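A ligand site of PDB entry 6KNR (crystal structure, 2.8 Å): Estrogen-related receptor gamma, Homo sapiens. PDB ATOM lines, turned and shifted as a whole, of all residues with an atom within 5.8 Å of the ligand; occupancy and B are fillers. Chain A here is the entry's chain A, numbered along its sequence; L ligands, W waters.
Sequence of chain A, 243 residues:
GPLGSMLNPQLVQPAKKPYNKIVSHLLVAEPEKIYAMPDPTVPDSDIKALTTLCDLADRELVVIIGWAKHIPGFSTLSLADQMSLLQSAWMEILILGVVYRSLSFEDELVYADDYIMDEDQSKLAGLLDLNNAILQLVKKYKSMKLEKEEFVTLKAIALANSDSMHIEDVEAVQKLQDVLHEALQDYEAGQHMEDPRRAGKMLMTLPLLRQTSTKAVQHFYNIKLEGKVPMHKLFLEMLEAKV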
ATOM      1  N   LEU A  50     -23.471 -21.635 -10.179  1.00  0.00           N
ATOM      2  CA  LEU A  50     -23.876 -23.019 -10.420  1.00  0.00           C
ATOM      3  C   LEU A  50     -25.244 -23.328  -9.826  1.00  0.00           C
ATOM      4  O   LEU A  50     -26.034 -24.036 -10.462  1.00  0.00           O
ATOM      5  CB  LEU A  50     -22.814 -23.981  -9.891  1.00  0.00           C
ATOM      6  CG  LEU A  50     -21.473 -23.868 -10.643  1.00  0.00           C
ATOM      7  CD1 LEU A  50     -20.434 -24.721  -9.977  1.00  0.00           C
ATOM      8  CD2 LEU A  50     -21.606 -24.256 -12.103  1.00  0.00           C
ATOM      9  N   LEU A  53     -27.738 -22.038 -12.221  1.00  0.00           N
ATOM     10  CA  LEU A  53     -27.926 -22.932 -13.337  1.00  0.00           C
ATOM     11  C   LEU A  53     -28.731 -24.167 -12.941  1.00  0.00           C
ATOM     12  O   LEU A  53     -29.494 -24.699 -13.761  1.00  0.00           O
ATOM     13  CB  LEU A  53     -26.568 -23.318 -13.931  1.00  0.00           C
ATOM     14  CG  LEU A  53     -25.886 -22.205 -14.742  1.00  0.00           C
ATOM     15  CD1 LEU A  53     -24.419 -22.534 -15.019  1.00  0.00           C
ATOM     16  CD2 LEU A  53     -26.614 -21.857 -16.053  1.00  0.00           C
ATOM     17  N   CYS A  54     -28.612 -24.643 -11.703  1.00  0.00           N
ATOM     18  CA  CYS A  54     -29.387 -25.840 -11.321  1.00  0.00           C
ATOM     19  C   CYS A  54     -30.874 -25.512 -11.236  1.00  0.00           C
ATOM     20  O   CYS A  54     -31.706 -26.279 -11.724  1.00  0.00           O
ATOM     21  CB  CYS A  54     -28.904 -26.439  -9.998  1.00  0.00           C
ATOM     22  SG  CYS A  54     -27.313 -27.357 -10.093  1.00  0.00           S
ATOM     23  N   LEU A  56     -32.497 -23.064 -12.750  1.00  0.00           N
ATOM     24  CA  LEU A  56     -32.894 -22.874 -14.140  1.00  0.00           C
ATOM     25  C   LEU A  56     -33.179 -24.211 -14.827  1.00  0.00           C
ATOM     26  O   LEU A  56     -34.227 -24.390 -15.476  1.00  0.00           O
ATOM     27  CB  LEU A  56     -31.805 -22.108 -14.879  1.00  0.00           C
ATOM     28  CG  LEU A  56     -32.164 -21.887 -16.356  1.00  0.00           C
ATOM     29  CD1 LEU A  56     -33.458 -21.096 -16.475  1.00  0.00           C
ATOM     30  CD2 LEU A  56     -31.048 -21.180 -17.092  1.00  0.00           C
ATOM     31  N   ALA A  57     -32.250 -25.165 -14.710  1.00  0.00           N
ATOM     32  CA  ALA A  57     -32.372 -26.406 -15.474  1.00  0.00           C
ATOM     33  C   ALA A  57     -33.534 -27.260 -14.986  1.00  0.00           C
ATOM     34  O   ALA A  57     -34.169 -27.953 -15.791  1.00  0.00           O
ATOM     35  CB  ALA A  57     -31.076 -27.215 -15.401  1.00  0.00           C
ATOM     36  N   ASP A  58     -33.810 -27.254 -13.678  1.00  0.00           N
ATOM     37  CA  ASP A  58     -34.923 -28.052 -13.188  1.00  0.00           C
ATOM     38  C   ASP A  58     -36.259 -27.489 -13.656  1.00  0.00           C
ATOM     39  O   ASP A  58     -37.187 -28.237 -13.973  1.00  0.00           O
ATOM     40  CB  ASP A  58     -34.875 -28.145 -11.667  1.00  0.00           C
ATOM     41  CG  ASP A  58     -33.778 -29.089 -11.161  1.00  0.00           C
ATOM     42  OD1 ASP A  58     -33.178 -29.823 -11.987  1.00  0.00           O
ATOM     43  OD2 ASP A  58     -33.515 -29.100  -9.931  1.00  0.00           O
ATOM     44  N   GLU A  60     -36.591 -25.992 -16.516  1.00  0.00           N
ATOM     45  CA  GLU A  60     -36.624 -26.411 -17.919  1.00  0.00           C
ATOM     46  C   GLU A  60     -36.970 -27.885 -18.060  1.00  0.00           C
ATOM     47  O   GLU A  60     -37.697 -28.258 -18.984  1.00  0.00           O
ATOM     48  CB  GLU A  60     -35.285 -26.145 -18.579  1.00  0.00           C
ATOM     49  CG  GLU A  60     -35.034 -24.707 -18.852  1.00  0.00           C
ATOM     50  CD  GLU A  60     -33.780 -24.524 -19.673  1.00  0.00           C
ATOM     51  OE1 GLU A  60     -32.730 -24.266 -19.058  1.00  0.00           O
ATOM     52  OE2 GLU A  60     -33.870 -24.656 -20.920  1.00  0.00           O
ATOM     53  N   LEU A  61     -36.426 -28.737 -17.187  1.00  0.00           N
ATOM     54  CA  LEU A  61     -36.777 -30.149 -17.244  1.00  0.00           C
ATOM     55  C   LEU A  61     -38.282 -30.360 -17.076  1.00  0.00           C
ATOM     56  O   LEU A  61     -38.882 -31.215 -17.742  1.00  0.00           O
ATOM     57  CB  LEU A  61     -35.991 -30.943 -16.196  1.00  0.00           C
ATOM     58  CG  LEU A  61     -34.506 -31.039 -16.518  1.00  0.00           C
ATOM     59  CD1 LEU A  61     -33.748 -31.735 -15.410  1.00  0.00           C
ATOM     60  CD2 LEU A  61     -34.263 -31.731 -17.857  1.00  0.00           C
ATOM     61  N   TRP A  90     -31.891 -35.788 -21.828  1.00  0.00           N
ATOM     62  CA  TRP A  90     -32.297 -34.489 -21.283  1.00  0.00           C
ATOM     63  C   TRP A  90     -31.174 -33.459 -21.371  1.00  0.00           C
ATOM     64  O   TRP A  90     -31.426 -32.296 -21.668  1.00  0.00           O
ATOM     65  CB  TRP A  90     -32.798 -34.630 -19.848  1.00  0.00           C
ATOM     66  CG  TRP A  90     -31.830 -35.123 -18.854  1.00  0.00           C
ATOM     67  CD1 TRP A  90     -31.698 -36.409 -18.429  1.00  0.00           C
ATOM     68  CD2 TRP A  90     -30.859 -34.350 -18.124  1.00  0.00           C
ATOM     69  NE1 TRP A  90     -30.703 -36.489 -17.479  1.00  0.00           N
ATOM     70  CE2 TRP A  90     -30.178 -35.240 -17.276  1.00  0.00           C
ATOM     71  CE3 TRP A  90     -30.495 -33.007 -18.120  1.00  0.00           C
ATOM     72  CZ2 TRP A  90     -29.152 -34.823 -16.421  1.00  0.00           C
ATOM     73  CZ3 TRP A  90     -29.481 -32.595 -17.269  1.00  0.00           C
ATOM     74  CH2 TRP A  90     -28.818 -33.502 -16.438  1.00  0.00           C
ATOM     75  N   MET A  91     -29.931 -33.869 -21.155  1.00  0.00           N
ATOM     76  CA  MET A  91     -28.846 -32.907 -21.257  1.00  0.00           C
ATOM     77  C   MET A  91     -28.629 -32.481 -22.707  1.00  0.00           C
ATOM     78  O   MET A  91     -28.331 -31.320 -22.983  1.00  0.00           O
ATOM     79  CB  MET A  91     -27.589 -33.477 -20.612  1.00  0.00           C
ATOM     80  CG  MET A  91     -26.400 -32.549 -20.546  1.00  0.00           C
ATOM     81  SD  MET A  91     -26.695 -30.997 -19.686  1.00  0.00           S
ATOM     82  CE  MET A  91     -26.222 -31.503 -18.021  1.00  0.00           C
ATOM     83  N   LEU A  94     -31.270 -29.860 -23.221  1.00  0.00           N
ATOM     84  CA  LEU A  94     -30.938 -28.608 -22.555  1.00  0.00           C
ATOM     85  C   LEU A  94     -29.867 -27.845 -23.306  1.00  0.00           C
ATOM     86  O   LEU A  94     -30.000 -26.644 -23.570  1.00  0.00           O
ATOM     87  CB  LEU A  94     -30.477 -28.846 -21.122  1.00  0.00           C
ATOM     88  CG  LEU A  94     -31.551 -29.212 -20.126  1.00  0.00           C
ATOM     89  CD1 LEU A  94     -30.908 -29.426 -18.779  1.00  0.00           C
ATOM     90  CD2 LEU A  94     -32.613 -28.139 -20.095  1.00  0.00           C
ATOM     91  N   ILE A  95     -28.776 -28.530 -23.663  1.00  0.00           N
ATOM     92  CA  ILE A  95     -27.645 -27.852 -24.301  1.00  0.00           C
ATOM     93  C   ILE A  95     -28.046 -27.334 -25.670  1.00  0.00           C
ATOM     94  O   ILE A  95     -27.691 -26.218 -26.054  1.00  0.00           O
ATOM     95  CB  ILE A  95     -26.436 -28.797 -24.388  1.00  0.00           C
ATOM     96  CG1 ILE A  95     -25.735 -28.869 -23.038  1.00  0.00           C
ATOM     97  CG2 ILE A  95     -25.486 -28.358 -25.490  1.00  0.00           C
ATOM     98  CD1 ILE A  95     -24.949 -30.140 -22.863  1.00  0.00           C
ATOM     99  N   VAL A  98     -29.586 -23.974 -25.227  1.00  0.00           N
ATOM    100  CA  VAL A  98     -28.583 -22.933 -25.037  1.00  0.00           C
ATOM    101  C   VAL A  98     -27.902 -22.614 -26.360  1.00  0.00           C
ATOM    102  O   VAL A  98     -27.688 -21.445 -26.723  1.00  0.00           O
ATOM    103  CB  VAL A  98     -27.545 -23.355 -23.988  1.00  0.00           C
ATOM    104  CG1 VAL A  98     -26.477 -22.296 -23.897  1.00  0.00           C
ATOM    105  CG2 VAL A  98     -28.192 -23.581 -22.630  1.00  0.00           C
ATOM    106  N   ARG A 101     -30.261 -20.414 -28.473  1.00  0.00           N
ATOM    107  CA  ARG A 101     -30.429 -19.043 -27.980  1.00  0.00           C
ATOM    108  C   ARG A 101     -29.196 -18.177 -28.171  1.00  0.00           C
ATOM    109  O   ARG A 101     -29.293 -16.950 -28.029  1.00  0.00           O
ATOM    110  CB  ARG A 101     -30.838 -19.059 -26.509  1.00  0.00           C
ATOM    111  CG  ARG A 101     -32.047 -19.900 -26.200  1.00  0.00           C
ATOM    112  CD  ARG A 101     -32.530 -19.677 -24.779  1.00  0.00           C
ATOM    113  NE  ARG A 101     -31.761 -20.422 -23.783  1.00  0.00           N
ATOM    114  CZ  ARG A 101     -31.997 -21.688 -23.440  1.00  0.00           C
ATOM    115  NH1 ARG A 101     -32.974 -22.352 -24.033  1.00  0.00           N
ATOM    116  NH2 ARG A 101     -31.249 -22.285 -22.519  1.00  0.00           N
ATOM    117  N   LEU A 109     -22.728 -17.499 -24.105  1.00  0.00           N
ATOM    118  CA  LEU A 109     -23.764 -18.518 -24.018  1.00  0.00           C
ATOM    119  C   LEU A 109     -24.990 -17.912 -23.368  1.00  0.00           C
ATOM    120  O   LEU A 109     -24.920 -17.445 -22.227  1.00  0.00           O
ATOM    121  CB  LEU A 109     -23.288 -19.723 -23.207  1.00  0.00           C
ATOM    122  CG  LEU A 109     -22.285 -20.559 -23.986  1.00  0.00           C
ATOM    123  CD1 LEU A 109     -22.011 -21.850 -23.233  1.00  0.00           C
ATOM    124  CD2 LEU A 109     -22.792 -20.798 -25.412  1.00  0.00           C
ATOM    125  N   TYR A 111     -27.984 -18.572 -21.624  1.00  0.00           N
ATOM    126  CA  TYR A 111     -28.756 -19.554 -20.865  1.00  0.00           C
ATOM    127  C   TYR A 111     -30.210 -19.134 -20.745  1.00  0.00           C
ATOM    128  O   TYR A 111     -31.120 -19.975 -20.840  1.00  0.00           O
ATOM    129  CB  TYR A 111     -28.169 -19.751 -19.483  1.00  0.00           C
ATOM    130  CG  TYR A 111     -26.822 -20.445 -19.421  1.00  0.00           C
ATOM    131  CD1 TYR A 111     -25.660 -19.706 -19.277  1.00  0.00           C
ATOM    132  CD2 TYR A 111     -26.721 -21.834 -19.451  1.00  0.00           C
ATOM    133  CE1 TYR A 111     -24.430 -20.312 -19.191  1.00  0.00           C
ATOM    134  CE2 TYR A 111     -25.487 -22.464 -19.388  1.00  0.00           C
ATOM    135  CZ  TYR A 111     -24.352 -21.689 -19.240  1.00  0.00           C
ATOM    136  OH  TYR A 111     -23.109 -22.262 -19.143  1.00  0.00           O
ATOM    137  N   LEU A 127     -16.461 -23.201 -15.746  1.00  0.00           N
ATOM    138  CA  LEU A 127     -17.087 -23.809 -16.914  1.00  0.00           C
ATOM    139  C   LEU A 127     -16.398 -23.455 -18.233  1.00  0.00           C
ATOM    140  O   LEU A 127     -16.970 -23.674 -19.305  1.00  0.00           O
ATOM    141  CB  LEU A 127     -18.571 -23.400 -16.966  1.00  0.00           C
ATOM    142  CG  LEU A 127     -19.450 -23.741 -15.766  1.00  0.00           C
ATOM    143  CD1 LEU A 127     -20.728 -22.947 -15.805  1.00  0.00           C
ATOM    144  CD2 LEU A 127     -19.731 -25.222 -15.753  1.00  0.00           C
ATOM    145  N   LEU A 130     -15.920 -26.470 -20.710  1.00  0.00           N
ATOM    146  CA  LEU A 130     -17.224 -26.946 -21.130  1.00  0.00           C
ATOM    147  C   LEU A 130     -17.882 -25.950 -22.072  1.00  0.00           C
ATOM    148  O   LEU A 130     -18.372 -26.311 -23.140  1.00  0.00           O
ATOM    149  CB  LEU A 130     -18.087 -27.212 -19.910  1.00  0.00           C
ATOM    150  CG  LEU A 130     -19.490 -27.730 -20.185  1.00  0.00           C
ATOM    151  CD1 LEU A 130     -19.451 -28.925 -21.128  1.00  0.00           C
ATOM    152  CD2 LEU A 130     -20.178 -28.084 -18.865  1.00  0.00           C
ATOM    153  N   ASN A 131     -17.873 -24.665 -21.687  1.00  0.00           N
ATOM    154  CA  ASN A 131     -18.532 -23.670 -22.525  1.00  0.00           C
ATOM    155  C   ASN A 131     -17.822 -23.482 -23.852  1.00  0.00           C
ATOM    156  O   ASN A 131     -18.474 -23.176 -24.857  1.00  0.00           O
ATOM    157  CB  ASN A 131     -18.633 -22.360 -21.763  1.00  0.00           C
ATOM    158  CG  ASN A 131     -19.739 -22.408 -20.725  1.00  0.00           C
ATOM    159  OD1 ASN A 131     -20.479 -23.369 -20.673  1.00  0.00           O
ATOM    160  ND2 ASN A 131     -19.841 -21.379 -19.903  1.00  0.00           N
ATOM    161  N   ILE A 134     -19.300 -26.071 -26.085  1.00  0.00           N
ATOM    162  CA  ILE A 134     -20.629 -25.664 -26.532  1.00  0.00           C
ATOM    163  C   ILE A 134     -20.522 -24.599 -27.630  1.00  0.00           C
ATOM    164  O   ILE A 134     -21.218 -24.658 -28.641  1.00  0.00           O
ATOM    165  CB  ILE A 134     -21.464 -25.166 -25.335  1.00  0.00           C
ATOM    166  CG1 ILE A 134     -21.665 -26.300 -24.337  1.00  0.00           C
ATOM    167  CG2 ILE A 134     -22.824 -24.689 -25.766  1.00  0.00           C
ATOM    168  CD1 ILE A 134     -22.687 -25.985 -23.286  1.00  0.00           C
ATOM    169  N   ALA A 216     -20.671 -32.436 -20.064  1.00  0.00           N
ATOM    170  CA  ALA A 216     -21.431 -31.730 -19.041  1.00  0.00           C
ATOM    171  C   ALA A 216     -21.867 -32.670 -17.913  1.00  0.00           C
ATOM    172  O   ALA A 216     -21.743 -32.347 -16.722  1.00  0.00           O
ATOM    173  CB  ALA A 216     -22.635 -31.022 -19.666  1.00  0.00           C
ATOM    174  N   VAL A 217     -22.406 -33.834 -18.239  1.00  0.00           N
ATOM    175  CA  VAL A 217     -22.836 -34.714 -17.153  1.00  0.00           C
ATOM    176  C   VAL A 217     -21.635 -35.147 -16.325  1.00  0.00           C
ATOM    177  O   VAL A 217     -21.704 -35.214 -15.096  1.00  0.00           O
ATOM    178  CB  VAL A 217     -23.646 -35.914 -17.689  1.00  0.00           C
ATOM    179  CG1 VAL A 217     -23.843 -36.918 -16.584  1.00  0.00           C
ATOM    180  CG2 VAL A 217     -24.988 -35.436 -18.226  1.00  0.00           C
ATOM    181  N   HIS A 219     -19.192 -33.378 -15.603  1.00  0.00           N
ATOM    182  CA  HIS A 219     -18.759 -32.300 -14.723  1.00  0.00           C
ATOM    183  C   HIS A 219     -19.462 -32.350 -13.366  1.00  0.00           C
ATOM    184  O   HIS A 219     -18.876 -31.966 -12.355  1.00  0.00           O
ATOM    185  CB  HIS A 219     -18.979 -30.946 -15.373  1.00  0.00           C
ATOM    186  CG  HIS A 219     -18.269 -29.825 -14.687  1.00  0.00           C
ATOM    187  ND1 HIS A 219     -16.964 -29.930 -14.260  1.00  0.00           N
ATOM    188  CD2 HIS A 219     -18.686 -28.590 -14.343  1.00  0.00           C
ATOM    189  CE1 HIS A 219     -16.605 -28.797 -13.683  1.00  0.00           C
ATOM    190  NE2 HIS A 219     -17.628 -27.956 -13.730  1.00  0.00           N
ATOM    191  N   PHE A 220     -20.711 -32.834 -13.325  1.00  0.00           N
ATOM    192  CA  PHE A 220     -21.396 -33.048 -12.051  1.00  0.00           C
ATOM    193  C   PHE A 220     -20.493 -33.765 -11.049  1.00  0.00           C
ATOM    194  O   PHE A 220     -20.574 -33.514  -9.845  1.00  0.00           O
ATOM    195  CB  PHE A 220     -22.668 -33.865 -12.245  1.00  0.00           C
ATOM    196  CG  PHE A 220     -23.737 -33.128 -12.968  1.00  0.00           C
ATOM    197  CD1 PHE A 220     -24.121 -31.857 -12.564  1.00  0.00           C
ATOM    198  CD2 PHE A 220     -24.364 -33.690 -14.084  1.00  0.00           C
ATOM    199  CE1 PHE A 220     -25.113 -31.159 -13.228  1.00  0.00           C
ATOM    200  CE2 PHE A 220     -25.351 -32.998 -14.754  1.00  0.00           C
ATOM    201  CZ  PHE A 220     -25.721 -31.708 -14.304  1.00  0.00           C
ATOM    202  N   ILE A 223     -17.918 -31.415  -9.427  1.00  0.00           N
ATOM    203  CA  ILE A 223     -18.601 -30.553  -8.503  1.00  0.00           C
ATOM    204  C   ILE A 223     -18.903 -31.321  -7.229  1.00  0.00           C
ATOM    205  O   ILE A 223     -18.712 -30.817  -6.123  1.00  0.00           O
ATOM    206  CB  ILE A 223     -19.875 -29.974  -9.157  1.00  0.00           C
ATOM    207  CG1 ILE A 223     -19.501 -28.941 -10.200  1.00  0.00           C
ATOM    208  CG2 ILE A 223     -20.765 -29.359  -8.121  1.00  0.00           C
ATOM    209  CD1 ILE A 223     -20.644 -28.549 -11.122  1.00  0.00           C
ATOM    210  N   HIS A 232     -28.953 -30.984  -4.410  1.00  0.00           N
ATOM    211  CA  HIS A 232     -30.121 -31.645  -3.842  1.00  0.00           C
ATOM    212  C   HIS A 232     -29.816 -33.110  -3.533  1.00  0.00           C
ATOM    213  O   HIS A 232     -29.125 -33.798  -4.290  1.00  0.00           O
ATOM    214  CB  HIS A 232     -31.306 -31.544  -4.818  1.00  0.00           C
ATOM    215  CG  HIS A 232     -32.625 -31.956  -4.223  1.00  0.00           C
ATOM    216  ND1 HIS A 232     -33.031 -33.264  -4.147  1.00  0.00           N
ATOM    217  CD2 HIS A 232     -33.625 -31.213  -3.690  1.00  0.00           C
ATOM    218  CE1 HIS A 232     -34.222 -33.323  -3.576  1.00  0.00           C
ATOM    219  NE2 HIS A 232     -34.613 -32.091  -3.293  1.00  0.00           N
ATOM    220  N   PHE A 235     -30.514 -35.589  -6.248  1.00  0.00           N
ATOM    221  CA  PHE A 235     -29.512 -35.532  -7.305  1.00  0.00           C
ATOM    222  C   PHE A 235     -28.246 -36.307  -6.914  1.00  0.00           C
ATOM    223  O   PHE A 235     -27.740 -37.120  -7.687  1.00  0.00           O
ATOM    224  CB  PHE A 235     -29.194 -34.077  -7.639  1.00  0.00           C
ATOM    225  CG  PHE A 235     -28.419 -33.910  -8.919  1.00  0.00           C
ATOM    226  CD1 PHE A 235     -28.713 -34.705 -10.031  1.00  0.00           C
ATOM    227  CD2 PHE A 235     -27.404 -32.972  -9.024  1.00  0.00           C
ATOM    228  CE1 PHE A 235     -28.009 -34.550 -11.206  1.00  0.00           C
ATOM    229  CE2 PHE A 235     -26.676 -32.820 -10.192  1.00  0.00           C
ATOM    230  CZ  PHE A 235     -26.970 -33.620 -11.280  1.00  0.00           C
ATOM    231  N   MET A 238     -28.889 -39.914  -7.339  1.00  0.00           N
ATOM    232  CA  MET A 238     -28.845 -40.264  -8.746  1.00  0.00           C
ATOM    233  C   MET A 238     -27.413 -40.313  -9.274  1.00  0.00           C
ATOM    234  O   MET A 238     -27.042 -41.239  -9.995  1.00  0.00           O
ATOM    235  CB  MET A 238     -29.677 -39.272  -9.565  1.00  0.00           C
ATOM    236  CG  MET A 238     -31.120 -39.176  -9.082  1.00  0.00           C
ATOM    237  SD  MET A 238     -32.242 -38.312 -10.185  1.00  0.00           S
ATOM    238  CE  MET A 238     -31.469 -36.706 -10.177  1.00  0.00           C
HETATM  239  N1  LIG L   1     -31.165 -31.702 -11.413  1.00  0.00           N
HETATM  240  C1  LIG L   1     -25.195 -26.684 -16.786  1.00  0.00           C
HETATM  241  C2  LIG L   1     -24.230 -27.507 -15.976  1.00  0.00           C
HETATM  242  C3  LIG L   1     -24.158 -28.885 -16.150  1.00  0.00           C
HETATM  243  C4  LIG L   1     -23.275 -29.644 -15.416  1.00  0.00           C
HETATM  244  C5  LIG L   1     -22.469 -29.052 -14.484  1.00  0.00           C
HETATM  245  C6  LIG L   1     -23.402 -26.926 -15.027  1.00  0.00           C
HETATM  246  C7  LIG L   1     -27.535 -26.535 -19.033  1.00  0.00           C
HETATM  247  C8  LIG L   1     -29.425 -25.085 -19.321  1.00  0.00           C
HETATM  248  C9  LIG L   1     -28.482 -25.382 -17.154  1.00  0.00           C
HETATM  249  C10 LIG L   1     -27.689 -28.411 -13.542  1.00  0.00           C
HETATM  250  C11 LIG L   1     -28.504 -29.432 -13.964  1.00  0.00           C
HETATM  251  C12 LIG L   1     -28.807 -29.529 -15.321  1.00  0.00           C
HETATM  252  C13 LIG L   1     -29.219 -30.196 -12.883  1.00  0.00           C
HETATM  253  C14 LIG L   1     -30.770 -32.204 -12.733  1.00  0.00           C
HETATM  254  C15 LIG L   1     -28.780 -30.996 -11.694  1.00  0.00           C
HETATM  255  C16 LIG L   1     -23.161 -25.530 -19.829  1.00  0.00           C
HETATM  256  C17 LIG L   1     -26.527 -26.886 -16.764  1.00  0.00           C
HETATM  257  C18 LIG L   1     -27.509 -26.244 -17.671  1.00  0.00           C
HETATM  258  C19 LIG L   1     -28.482 -25.957 -19.855  1.00  0.00           C
HETATM  259  C20 LIG L   1     -29.422 -24.792 -17.965  1.00  0.00           C
HETATM  260  C21 LIG L   1     -27.240 -27.762 -15.804  1.00  0.00           C
HETATM  261  C22 LIG L   1     -27.027 -27.604 -14.439  1.00  0.00           C
HETATM  262  C23 LIG L   1     -23.701 -26.419 -18.748  1.00  0.00           C
HETATM  263  C24 LIG L   1     -28.152 -28.725 -16.240  1.00  0.00           C
HETATM  264  C25 LIG L   1     -30.390 -30.983 -13.539  1.00  0.00           C
HETATM  265  C26 LIG L   1     -29.996 -31.079 -10.773  1.00  0.00           C
HETATM  266  C27 LIG L   1     -31.797 -32.705 -10.589  1.00  0.00           C
HETATM  267  C28 LIG L   1     -24.540 -25.683 -17.708  1.00  0.00           C
HETATM  268  C29 LIG L   1     -32.719 -32.202  -9.529  1.00  0.00           C
HETATM  269  C30 LIG L   1     -33.274 -32.902 -10.723  1.00  0.00           C
HETATM  270  C31 LIG L   1     -22.536 -27.694 -14.282  1.00  0.00           C
HETATM  271  O1  LIG L   1     -22.047 -24.794 -19.362  1.00  0.00           O
HETATM  272  O2  LIG L   1     -30.359 -24.511 -20.127  1.00  0.00           O
HETATM  273  O   HOH W   1     -32.126 -25.072 -22.797  1.00  0.00           O
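OD1 of Asn 131 is in hydrogen-bond range of O1 of the ligand (2.5 Å).
OE1 of Glu 60 lies within hydrogen-bond range of O2 of the ligand, 2.6 Å away.
An oxygen (O1) of the ligand is in hydrogen-bond range of the side-chain hydroxyl of Tyr 111, at 2.8 Å.
OD1 of Asp 58 is in salt-bridge range of N1 of the ligand (2.8 Å).
The guanidinium group of Arg 101 sits at hydrogen-bond distance from an oxygen (O2) of the ligand (3.4 Å).
Water W1 lies within hydrogen-bond range of the side-chain carboxylate of Glu 60, the backbone carbonyl oxygen of Leu 94, the guanidinium group of Arg 101 and an oxygen (O2) of the ligand.
The side-chain amide oxygen (OD1) of Asn 131 is in hydrogen-bond range of the side-chain hydroxyl (OH) of Tyr 111, at 3.2 Å.
The guanidinium group of Arg 101 is in salt-bridge range of the side-chain carboxylate of Glu 60 (3.9 Å).
O of Tyr 111 sits at hydrogen-bond distance from NH2 of Arg 101.
The backbone carbonyl oxygen of Leu 50 lies within hydrogen-bond range of the side-chain sulfur of Cys 54, at 3.6 Å.
Leu 53 touches the ligand.
Cys 54 touches the ligand.
CB of Ala 57 touches C12 of the ligand, 3.2 Å away.
Leu 61 touches the ligand (CD1 to C25, 3.9 Å).
CZ3 of Trp 90 touches C12 of the ligand, at 3.7 Å.
CE of Met 91 touches C24 of the ligand, 3.8 Å away.
Leu 94 touches the ligand.
CG2 of Val 98 touches O2 of the ligand, at 3.4 Å.
Leu 130 touches the ligand (CD2 to O1, 3.8 Å).
Ile 134 touches the ligand (CD1 to C16, 3.5 Å).
Ala 216 touches the ligand.
CD2 of His 219 touches C5 of the ligand, at 3.8 Å.
Phe 220 touches the ligand.
Ile 223 touches the ligand.
Phe 235 touches the ligand (CE2 to C15, 3.2 Å).
Hydrophobic or aromatic side chains within 4 Å of the ligand: Ala 57, Leu 61, Trp 90, Met 91, Leu 94, Val 98, Tyr 111, Leu 130, Ile 134, His 219, Phe 220, Ile 223 and Phe 235.
20 residues have an atom within 4 Å of the ligand: Leu 53, Cys 54, Ala 57, Asp 58, Glu 60, Leu 61, Trp 90, Met 91, Leu 94, Val 98, Arg 101, Tyr 111, Leu 130, Asn 131, Ile 134, Ala 216, His 219, Phe 220, Ile 223 and Phe 235.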
